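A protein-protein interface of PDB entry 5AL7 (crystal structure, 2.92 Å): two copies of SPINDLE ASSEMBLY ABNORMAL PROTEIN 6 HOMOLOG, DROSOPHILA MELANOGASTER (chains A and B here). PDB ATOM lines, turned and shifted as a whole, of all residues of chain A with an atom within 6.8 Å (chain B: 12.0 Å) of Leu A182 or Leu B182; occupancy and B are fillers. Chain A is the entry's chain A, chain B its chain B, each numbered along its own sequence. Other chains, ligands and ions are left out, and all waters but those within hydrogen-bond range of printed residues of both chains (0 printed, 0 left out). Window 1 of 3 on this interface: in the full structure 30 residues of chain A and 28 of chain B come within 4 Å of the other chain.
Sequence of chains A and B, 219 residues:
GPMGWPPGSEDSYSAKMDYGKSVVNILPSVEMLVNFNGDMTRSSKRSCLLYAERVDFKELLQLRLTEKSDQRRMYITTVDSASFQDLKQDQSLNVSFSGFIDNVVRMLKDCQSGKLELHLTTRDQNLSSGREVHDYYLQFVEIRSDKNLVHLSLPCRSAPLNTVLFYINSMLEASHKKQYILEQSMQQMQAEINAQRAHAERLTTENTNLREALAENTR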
ATOM      1  N   HIS A 176      11.669  34.983  36.098  1.00  0.00           N
ATOM      2  CA  HIS A 176      10.820  33.803  36.134  1.00  0.00           C
ATOM      3  C   HIS A 176       9.931  33.728  34.905  1.00  0.00           C
ATOM      4  O   HIS A 176       9.804  32.658  34.309  1.00  0.00           O
ATOM      5  CB  HIS A 176       9.973  33.784  37.401  1.00  0.00           C
ATOM      6  CG  HIS A 176      10.719  33.319  38.609  1.00  0.00           C
ATOM      7  ND1 HIS A 176      10.253  33.509  39.892  1.00  0.00           N
ATOM      8  CD2 HIS A 176      11.903  32.671  38.729  1.00  0.00           C
ATOM      9  CE1 HIS A 176      11.116  32.994  40.752  1.00  0.00           C
ATOM     10  NE2 HIS A 176      12.127  32.482  40.071  1.00  0.00           N
ATOM     11  N   LYS A 177       9.354  34.860  34.503  1.00  0.00           N
ATOM     12  CA  LYS A 177       8.517  34.880  33.306  1.00  0.00           C
ATOM     13  C   LYS A 177       9.341  34.488  32.085  1.00  0.00           C
ATOM     14  O   LYS A 177       8.873  33.733  31.233  1.00  0.00           O
ATOM     15  CB  LYS A 177       7.873  36.249  33.095  1.00  0.00           C
ATOM     16  CG  LYS A 177       6.791  36.598  34.102  1.00  0.00           C
ATOM     17  CD  LYS A 177       6.037  37.852  33.685  1.00  0.00           C
ATOM     18  CE  LYS A 177       5.504  38.601  34.896  1.00  0.00           C
ATOM     19  NZ  LYS A 177       6.594  39.370  35.557  1.00  0.00           N
ATOM     20  N   LYS A 178      10.567  34.999  32.005  1.00  0.00           N
ATOM     21  CA  LYS A 178      11.452  34.658  30.899  1.00  0.00           C
ATOM     22  C   LYS A 178      11.767  33.166  30.889  1.00  0.00           C
ATOM     23  O   LYS A 178      11.767  32.543  29.835  1.00  0.00           O
ATOM     24  CB  LYS A 178      12.749  35.468  30.965  1.00  0.00           C
ATOM     25  CG  LYS A 178      12.620  36.895  30.441  1.00  0.00           C
ATOM     26  CD  LYS A 178      13.974  37.595  30.350  1.00  0.00           C
ATOM     27  CE  LYS A 178      13.842  38.996  29.759  1.00  0.00           C
ATOM     28  NZ  LYS A 178      13.250  39.962  30.730  1.00  0.00           N
ATOM     29  N   GLN A 179      11.999  32.588  32.063  1.00  0.00           N
ATOM     30  CA  GLN A 179      12.278  31.157  32.172  1.00  0.00           C
ATOM     31  C   GLN A 179      11.074  30.352  31.697  1.00  0.00           C
ATOM     32  O   GLN A 179      11.225  29.322  31.048  1.00  0.00           O
ATOM     33  CB  GLN A 179      12.639  30.780  33.604  1.00  0.00           C
ATOM     34  CG  GLN A 179      14.084  31.054  33.946  1.00  0.00           C
ATOM     35  CD  GLN A 179      14.452  30.601  35.340  1.00  0.00           C
ATOM     36  OE1 GLN A 179      13.616  30.082  36.083  1.00  0.00           O
ATOM     37  NE2 GLN A 179      15.711  30.798  35.708  1.00  0.00           N
ATOM     38  N   TYR A 180       9.882  30.835  32.035  1.00  0.00           N
ATOM     39  CA  TYR A 180       8.642  30.189  31.621  1.00  0.00           C
ATOM     40  C   TYR A 180       8.482  30.230  30.109  1.00  0.00           C
ATOM     41  O   TYR A 180       8.148  29.222  29.487  1.00  0.00           O
ATOM     42  CB  TYR A 180       7.439  30.862  32.283  1.00  0.00           C
ATOM     43  CG  TYR A 180       6.134  30.143  32.048  1.00  0.00           C
ATOM     44  CD1 TYR A 180       5.783  29.028  32.800  1.00  0.00           C
ATOM     45  CD2 TYR A 180       5.246  30.583  31.071  1.00  0.00           C
ATOM     46  CE1 TYR A 180       4.581  28.368  32.583  1.00  0.00           C
ATOM     47  CE2 TYR A 180       4.042  29.932  30.847  1.00  0.00           C
ATOM     48  CZ  TYR A 180       3.716  28.825  31.606  1.00  0.00           C
ATOM     49  OH  TYR A 180       2.522  28.171  31.390  1.00  0.00           O
ATOM     50  N   ILE A 181       8.729  31.396  29.523  1.00  0.00           N
ATOM     51  CA  ILE A 181       8.648  31.557  28.074  1.00  0.00           C
ATOM     52  C   ILE A 181       9.676  30.650  27.388  1.00  0.00           C
ATOM     53  O   ILE A 181       9.376  30.033  26.372  1.00  0.00           O
ATOM     54  CB  ILE A 181       8.850  33.037  27.647  1.00  0.00           C
ATOM     55  CG1 ILE A 181       7.601  33.863  27.982  1.00  0.00           C
ATOM     56  CG2 ILE A 181       9.144  33.144  26.157  1.00  0.00           C
ATOM     57  CD1 ILE A 181       7.840  35.362  28.036  1.00  0.00           C
ATOM     58  N   LEU A 182      10.877  30.561  27.955  1.00  0.00           N
ATOM     59  CA  LEU A 182      11.943  29.728  27.398  1.00  0.00           C
ATOM     60  C   LEU A 182      11.561  28.249  27.440  1.00  0.00           C
ATOM     61  O   LEU A 182      11.673  27.536  26.436  1.00  0.00           O
ATOM     62  CB  LEU A 182      13.261  29.952  28.144  1.00  0.00           C
ATOM     63  CG  LEU A 182      14.026  31.247  27.840  1.00  0.00           C
ATOM     64  CD1 LEU A 182      15.338  31.323  28.615  1.00  0.00           C
ATOM     65  CD2 LEU A 182      14.280  31.389  26.351  1.00  0.00           C
ATOM     66  N   GLU A 183      11.112  27.794  28.606  1.00  0.00           N
ATOM     67  CA  GLU A 183      10.782  26.385  28.803  1.00  0.00           C
ATOM     68  C   GLU A 183       9.550  25.966  28.015  1.00  0.00           C
ATOM     69  O   GLU A 183       9.440  24.810  27.623  1.00  0.00           O
ATOM     70  CB  GLU A 183      10.558  26.087  30.286  1.00  0.00           C
ATOM     71  CG  GLU A 183      11.818  26.115  31.129  1.00  0.00           C
ATOM     72  CD  GLU A 183      11.533  25.902  32.601  1.00  0.00           C
ATOM     73  OE1 GLU A 183      10.967  26.816  33.240  1.00  0.00           O
ATOM     74  OE2 GLU A 183      11.877  24.821  33.118  1.00  0.00           O
ATOM     75  N   GLN A 184       8.615  26.892  27.806  1.00  0.00           N
ATOM     76  CA  GLN A 184       7.430  26.601  26.996  1.00  0.00           C
ATOM     77  C   GLN A 184       7.754  26.677  25.504  1.00  0.00           C
ATOM     78  O   GLN A 184       7.115  26.012  24.688  1.00  0.00           O
ATOM     79  CB  GLN A 184       6.269  27.539  27.326  1.00  0.00           C
ATOM     80  CG  GLN A 184       4.923  26.962  26.901  1.00  0.00           C
ATOM     81  CD  GLN A 184       3.776  27.942  27.031  1.00  0.00           C
ATOM     82  OE1 GLN A 184       3.833  28.889  27.815  1.00  0.00           O
ATOM     83  NE2 GLN A 184       2.719  27.716  26.259  1.00  0.00           N
ATOM     84  N   SER A 185       8.741  27.497  25.150  1.00  0.00           N
ATOM     85  CA  SER A 185       9.206  27.589  23.768  1.00  0.00           C
ATOM     86  C   SER A 185      10.036  26.353  23.471  1.00  0.00           C
ATOM     87  O   SER A 185      10.318  26.029  22.317  1.00  0.00           O
ATOM     88  CB  SER A 185      10.024  28.862  23.536  1.00  0.00           C
ATOM     89  OG  SER A 185      10.471  28.948  22.194  1.00  0.00           O
ATOM     90  N   MET A 186      10.431  25.672  24.540  1.00  0.00           N
ATOM     91  CA  MET A 186      11.147  24.417  24.432  1.00  0.00           C
ATOM     92  C   MET A 186      10.122  23.286  24.356  1.00  0.00           C
ATOM     93  O   MET A 186      10.305  22.315  23.623  1.00  0.00           O
ATOM     94  CB  MET A 186      12.086  24.231  25.619  1.00  0.00           C
ATOM     95  CG  MET A 186      13.085  23.109  25.456  1.00  0.00           C
ATOM     96  SD  MET A 186      14.096  22.948  26.934  1.00  0.00           S
ATOM     97  CE  MET A 186      12.828  22.603  28.153  1.00  0.00           C
ATOM     98  N   GLN A 187       9.048  23.430  25.130  1.00  0.00           N
ATOM     99  CA  GLN A 187       7.989  22.424  25.237  1.00  0.00           C
ATOM    100  C   GLN A 187       7.231  22.180  23.929  1.00  0.00           C
ATOM    101  O   GLN A 187       6.933  21.039  23.588  1.00  0.00           O
ATOM    102  CB  GLN A 187       6.996  22.823  26.334  1.00  0.00           C
ATOM    103  CG  GLN A 187       7.414  22.412  27.736  1.00  0.00           C
ATOM    104  CD  GLN A 187       6.365  22.753  28.776  1.00  0.00           C
ATOM    105  OE1 GLN A 187       6.437  23.797  29.426  1.00  0.00           O
ATOM    106  NE2 GLN A 187       5.380  21.878  28.933  1.00  0.00           N
ATOM    107  N   GLU B 173      19.925  35.683  41.552  1.00  0.00           N
ATOM    108  CA  GLU B 173      21.199  35.197  41.047  1.00  0.00           C
ATOM    109  C   GLU B 173      21.089  33.756  40.569  1.00  0.00           C
ATOM    110  O   GLU B 173      21.586  33.396  39.486  1.00  0.00           O
ATOM    111  CB  GLU B 173      22.265  35.335  42.123  1.00  0.00           C
ATOM    112  CG  GLU B 173      22.629  36.789  42.359  1.00  0.00           C
ATOM    113  CD  GLU B 173      23.678  36.981  43.414  1.00  0.00           C
ATOM    114  OE1 GLU B 173      23.931  36.028  44.180  1.00  0.00           O
ATOM    115  OE2 GLU B 173      24.226  38.100  43.491  1.00  0.00           O
ATOM    116  N   ALA B 174      20.399  32.939  41.355  1.00  0.00           N
ATOM    117  CA  ALA B 174      20.213  31.542  40.982  1.00  0.00           C
ATOM    118  C   ALA B 174      19.408  31.438  39.697  1.00  0.00           C
ATOM    119  O   ALA B 174      19.680  30.588  38.839  1.00  0.00           O
ATOM    120  CB  ALA B 174      19.536  30.787  42.092  1.00  0.00           C
ATOM    121  N   SER B 175      18.437  32.336  39.559  1.00  0.00           N
ATOM    122  CA  SER B 175      17.592  32.366  38.381  1.00  0.00           C
ATOM    123  C   SER B 175      18.419  32.709  37.156  1.00  0.00           C
ATOM    124  O   SER B 175      18.232  32.120  36.092  1.00  0.00           O
ATOM    125  CB  SER B 175      16.452  33.370  38.558  1.00  0.00           C
ATOM    126  OG  SER B 175      15.543  33.317  37.471  1.00  0.00           O
ATOM    127  N   HIS B 176      19.360  33.635  37.310  1.00  0.00           N
ATOM    128  CA  HIS B 176      20.218  34.010  36.192  1.00  0.00           C
ATOM    129  C   HIS B 176      21.108  32.852  35.772  1.00  0.00           C
ATOM    130  O   HIS B 176      21.248  32.575  34.567  1.00  0.00           O
ATOM    131  CB  HIS B 176      21.083  35.213  36.551  1.00  0.00           C
ATOM    132  CG  HIS B 176      20.358  36.517  36.475  1.00  0.00           C
ATOM    133  ND1 HIS B 176      20.854  37.677  37.027  1.00  0.00           N
ATOM    134  CD2 HIS B 176      19.164  36.837  35.924  1.00  0.00           C
ATOM    135  CE1 HIS B 176      20.002  38.663  36.804  1.00  0.00           C
ATOM    136  NE2 HIS B 176      18.968  38.179  36.140  1.00  0.00           N
ATOM    137  N   LYS B 177      21.672  32.147  36.756  1.00  0.00           N
ATOM    138  CA  LYS B 177      22.508  30.990  36.440  1.00  0.00           C
ATOM    139  C   LYS B 177      21.682  29.936  35.681  1.00  0.00           C
ATOM    140  O   LYS B 177      22.143  29.349  34.681  1.00  0.00           O
ATOM    141  CB  LYS B 177      23.113  30.385  37.706  1.00  0.00           C
ATOM    142  CG  LYS B 177      24.156  31.256  38.392  1.00  0.00           C
ATOM    143  CD  LYS B 177      24.903  30.476  39.472  1.00  0.00           C
ATOM    144  CE  LYS B 177      25.373  31.376  40.615  1.00  0.00           C
ATOM    145  NZ  LYS B 177      24.251  31.695  41.562  1.00  0.00           N
ATOM    146  N   LYS B 178      20.450  29.720  36.142  1.00  0.00           N
ATOM    147  CA  LYS B 178      19.558  28.777  35.480  1.00  0.00           C
ATOM    148  C   LYS B 178      19.232  29.200  34.047  1.00  0.00           C
ATOM    149  O   LYS B 178      19.218  28.365  33.150  1.00  0.00           O
ATOM    150  CB  LYS B 178      18.261  28.601  36.279  1.00  0.00           C
ATOM    151  CG  LYS B 178      18.385  27.662  37.481  1.00  0.00           C
ATOM    152  CD  LYS B 178      17.032  27.376  38.130  1.00  0.00           C
ATOM    153  CE  LYS B 178      17.157  26.381  39.286  1.00  0.00           C
ATOM    154  NZ  LYS B 178      17.756  26.993  40.508  1.00  0.00           N
ATOM    155  N   GLN B 179      18.996  30.490  33.825  1.00  0.00           N
ATOM    156  CA  GLN B 179      18.697  30.972  32.476  1.00  0.00           C
ATOM    157  C   GLN B 179      19.865  30.766  31.528  1.00  0.00           C
ATOM    158  O   GLN B 179      19.686  30.329  30.387  1.00  0.00           O
ATOM    159  CB  GLN B 179      18.348  32.460  32.480  1.00  0.00           C
ATOM    160  CG  GLN B 179      16.921  32.829  32.813  1.00  0.00           C
ATOM    161  CD  GLN B 179      16.681  34.332  32.677  1.00  0.00           C
ATOM    162  OE1 GLN B 179      16.746  35.079  33.660  1.00  0.00           O
ATOM    163  NE2 GLN B 179      16.415  34.782  31.449  1.00  0.00           N
ATOM    164  N   TYR B 180      21.069  31.061  32.007  1.00  0.00           N
ATOM    165  CA  TYR B 180      22.233  30.943  31.140  1.00  0.00           C
ATOM    166  C   TYR B 180      22.461  29.475  30.781  1.00  0.00           C
ATOM    167  O   TYR B 180      22.660  29.137  29.603  1.00  0.00           O
ATOM    168  CB  TYR B 180      23.472  31.550  31.802  1.00  0.00           C
ATOM    169  CG  TYR B 180      24.620  31.777  30.842  1.00  0.00           C
ATOM    170  CD1 TYR B 180      24.638  32.894  30.015  1.00  0.00           C
ATOM    171  CD2 TYR B 180      25.686  30.889  30.765  1.00  0.00           C
ATOM    172  CE1 TYR B 180      25.677  33.119  29.132  1.00  0.00           C
ATOM    173  CE2 TYR B 180      26.735  31.111  29.887  1.00  0.00           C
ATOM    174  CZ  TYR B 180      26.722  32.225  29.072  1.00  0.00           C
ATOM    175  OH  TYR B 180      27.760  32.445  28.196  1.00  0.00           O
ATOM    176  N   ILE B 181      22.381  28.601  31.785  1.00  0.00           N
ATOM    177  CA  ILE B 181      22.552  27.166  31.547  1.00  0.00           C
ATOM    178  C   ILE B 181      21.494  26.628  30.574  1.00  0.00           C
ATOM    179  O   ILE B 181      21.806  25.862  29.647  1.00  0.00           O
ATOM    180  CB  ILE B 181      22.475  26.363  32.873  1.00  0.00           C
ATOM    181  CG1 ILE B 181      23.730  26.590  33.720  1.00  0.00           C
ATOM    182  CG2 ILE B 181      22.276  24.877  32.605  1.00  0.00           C
ATOM    183  CD1 ILE B 181      23.549  26.234  35.185  1.00  0.00           C
ATOM    184  N   LEU B 182      20.255  27.070  30.766  1.00  0.00           N
ATOM    185  CA  LEU B 182      19.137  26.612  29.949  1.00  0.00           C
ATOM    186  C   LEU B 182      19.270  27.035  28.482  1.00  0.00           C
ATOM    187  O   LEU B 182      19.210  26.189  27.588  1.00  0.00           O
ATOM    188  CB  LEU B 182      17.813  27.126  30.541  1.00  0.00           C
ATOM    189  CG  LEU B 182      16.477  26.755  29.891  1.00  0.00           C
ATOM    190  CD1 LEU B 182      15.391  26.637  30.943  1.00  0.00           C
ATOM    191  CD2 LEU B 182      16.073  27.787  28.846  1.00  0.00           C
ATOM    192  N   GLU B 183      19.462  28.327  28.223  1.00  0.00           N
ATOM    193  CA  GLU B 183      19.517  28.784  26.833  1.00  0.00           C
ATOM    194  C   GLU B 183      20.800  28.338  26.129  1.00  0.00           C
ATOM    195  O   GLU B 183      20.802  28.124  24.906  1.00  0.00           O
ATOM    196  CB  GLU B 183      19.363  30.302  26.742  1.00  0.00           C
ATOM    197  CG  GLU B 183      20.491  31.107  27.342  1.00  0.00           C
ATOM    198  CD  GLU B 183      20.268  32.592  27.166  1.00  0.00           C
ATOM    199  OE1 GLU B 183      19.692  32.975  26.127  1.00  0.00           O
ATOM    200  OE2 GLU B 183      20.651  33.371  28.066  1.00  0.00           O
ATOM    201  N   GLN B 184      21.877  28.162  26.894  1.00  0.00           N
ATOM    202  CA  GLN B 184      23.122  27.708  26.288  1.00  0.00           C
ATOM    203  C   GLN B 184      23.037  26.226  25.942  1.00  0.00           C
ATOM    204  O   GLN B 184      23.639  25.779  24.963  1.00  0.00           O
ATOM    205  CB  GLN B 184      24.310  27.949  27.220  1.00  0.00           C
ATOM    206  CG  GLN B 184      25.658  27.973  26.515  1.00  0.00           C
ATOM    207  CD  GLN B 184      26.821  27.998  27.485  1.00  0.00           C
ATOM    208  OE1 GLN B 184      26.678  28.416  28.631  1.00  0.00           O
ATOM    209  NE2 GLN B 184      27.984  27.550  27.027  1.00  0.00           N
ATOM    210  N   SER B 185      22.288  25.464  26.734  1.00  0.00           N
ATOM    211  CA  SER B 185      22.064  24.061  26.400  1.00  0.00           C
ATOM    212  C   SER B 185      20.975  23.889  25.330  1.00  0.00           C
ATOM    213  O   SER B 185      20.889  22.842  24.681  1.00  0.00           O
ATOM    214  CB  SER B 185      21.694  23.271  27.658  1.00  0.00           C
ATOM    215  OG  SER B 185      21.480  21.903  27.360  1.00  0.00           O
ATOM    216  N   MET B 186      20.170  24.932  25.133  1.00  0.00           N
ATOM    217  CA  MET B 186      19.060  24.903  24.176  1.00  0.00           C
ATOM    218  C   MET B 186      19.400  25.326  22.740  1.00  0.00           C
ATOM    219  O   MET B 186      18.899  24.727  21.780  1.00  0.00           O
ATOM    220  CB  MET B 186      17.922  25.784  24.706  1.00  0.00           C
ATOM    221  CG  MET B 186      16.599  25.632  23.976  1.00  0.00           C
ATOM    222  SD  MET B 186      15.336  26.738  24.637  1.00  0.00           S
ATOM    223  CE  MET B 186      14.016  26.504  23.447  1.00  0.00           C
ATOM    224  N   GLN B 187      20.244  26.345  22.591  1.00  0.00           N
ATOM    225  CA  GLN B 187      20.550  26.890  21.260  1.00  0.00           C
ATOM    226  C   GLN B 187      21.210  25.886  20.305  1.00  0.00           C
ATOM    227  O   GLN B 187      20.859  25.816  19.115  1.00  0.00           O
ATOM    228  CB  GLN B 187      21.436  28.129  21.390  1.00  0.00           C
ATOM    229  CG  GLN B 187      20.656  29.403  21.660  1.00  0.00           C
ATOM    230  CD  GLN B 187      21.537  30.633  21.686  1.00  0.00           C
ATOM    231  OE1 GLN B 187      22.705  30.566  22.061  1.00  0.00           O
ATOM    232  NE2 GLN B 187      20.977  31.769  21.287  1.00  0.00           N
ATOM    233  N   GLN B 188      22.150  25.101  20.825  1.00  0.00           N
ATOM    234  CA  GLN B 188      22.864  24.131  20.001  1.00  0.00           C
ATOM    235  C   GLN B 188      21.941  23.018  19.524  1.00  0.00           C
ATOM    236  O   GLN B 188      22.175  22.416  18.475  1.00  0.00           O
ATOM    237  CB  GLN B 188      24.032  23.522  20.776  1.00  0.00           C
ATOM    238  CG  GLN B 188      23.616  22.825  22.062  1.00  0.00           C
ATOM    239  CD  GLN B 188      24.758  22.073  22.709  1.00  0.00           C
ATOM    240  OE1 GLN B 188      25.923  22.285  22.378  1.00  0.00           O
ATOM    241  NE2 GLN B 188      24.428  21.181  23.635  1.00  0.00           N
ATOM    242  N   MET B 189      20.877  22.765  20.277  1.00  0.00           N
ATOM    243  CA  MET B 189      19.906  21.768  19.864  1.00  0.00           C
ATOM    244  C   MET B 189      18.900  22.409  18.919  1.00  0.00           C
ATOM    245  O   MET B 189      18.283  21.721  18.099  1.00  0.00           O
ATOM    246  CB  MET B 189      19.199  21.154  21.072  1.00  0.00           C
ATOM    247  CG  MET B 189      20.044  20.144  21.823  1.00  0.00           C
ATOM    248  SD  MET B 189      20.429  18.716  20.792  1.00  0.00           S
ATOM    249  CE  MET B 189      18.857  17.851  20.796  1.00  0.00           C
ATOM    250  N   GLN B 190      18.749  23.729  19.019  1.00  0.00           N
ATOM    251  CA  GLN B 190      17.857  24.440  18.110  1.00  0.00           C
ATOM    252  C   GLN B 190      18.503  24.546  16.728  1.00  0.00           C
ATOM    253  O   GLN B 190      17.811  24.691  15.717  1.00  0.00           O
ATOM    254  CB  GLN B 190      17.520  25.832  18.668  1.00  0.00           C
ATOM    255  CG  GLN B 190      16.661  26.713  17.759  1.00  0.00           C
ATOM    256  CD  GLN B 190      17.485  27.658  16.897  1.00  0.00           C
ATOM    257  OE1 GLN B 190      18.298  28.431  17.404  1.00  0.00           O
ATOM    258  NE2 GLN B 190      17.278  27.597  15.585  1.00  0.00           N
ATOM    259  N   ALA B 191      19.832  24.454  16.684  1.00  0.00           N
ATOM    260  CA  ALA B 191      20.539  24.355  15.405  1.00  0.00           C
ATOM    261  C   ALA B 191      20.674  22.892  14.967  1.00  0.00           C
ATOM    262  O   ALA B 191      20.701  22.575  13.766  1.00  0.00           O
ATOM    263  CB  ALA B 191      21.904  25.014  15.499  1.00  0.00           C
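NE2 of Gln A179 is in hydrogen-bond range of O of Ser B175 (2.9 Å).
His A176 touches Ser B175.
Gln B179 touches Lys A178.
Gln A179 touches Lys B178.
CG of Gln A179 touches CG of Gln B179, 3.5 Å away.
CB of Leu A182 touches CD2 of Leu B182 (3.6 Å).
Leu A182 touches Met B186.
CG of Glu A183 touches CD1 of Leu B182, at 3.6 Å.
O of Ser A185 touches CE of Met B186 (3.9 Å).
CA of Met A186 touches CE of Met B186, 3.7 Å away.
Of the printed residues of chain B, Lys A178 touches Gln B179.
Printed residues of chain B within 4 Å of Gln A179: Ser B175, Lys B178 and Gln B179.
No residue of chain B comes within 4 Å of Ile A181.
Leu A182 touches two residues of chain B.
Of the printed residues of chain B, Glu A183 touches Leu B182.
Ser A185 touches just one residue of chain B: Met B186 (3.9 Å).
Of chain B, only Met B186 (3.7 Å) comes within 4 Å of Met A186.
Printed residues of chain A within 4 Å of Lys B178: Gln A179 (3.4 Å).
Of the printed residues of chain A, Gln B179 touches Lys A178 (3.8 Å) and Gln A179 (3.5 Å).
Leu B182 touches just these residues of chain A: Leu A182 (3.6 Å) and Glu A183 (3.6 Å).
Gln B184 touches none of the printed residues of chain A.
Of the printed residues of chain A, Met B186 touches Leu A182 (3.9 Å), Ser A185 (3.9 Å) and Met A186 (3.7 Å).
The nearest residue of chain B that does not touch Leu A182 is Glu B183 (4.6 Å).
Hydrophobic or aromatic side chains of chain B that line the printed part of chain A: Leu B182 and Met B186.
Among the printed residues, 10 pairs touch across the chains.
Lys A178 touches Gln B179, and with the chains exchanged Gln A179 touches Lys B178.
Gln B179 touches its own counterpart, Gln A179.
Glu A183 touches Leu B182, but with the chains exchanged Leu A182 does not touch Glu B183 (4.6 Å).
Ser A185 touches Met B186, but with the chains exchanged Met A186 does not touch Ser B185 (7.1 Å).
Positions printed for both chains: 176, 177, 178, 179, 180, 181, 182, 183, 184, 185, 186 and 187.
Of the 10 pairs that touch across the chains among the printed residues, 5 have their exchanged pair printed and touching as well.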
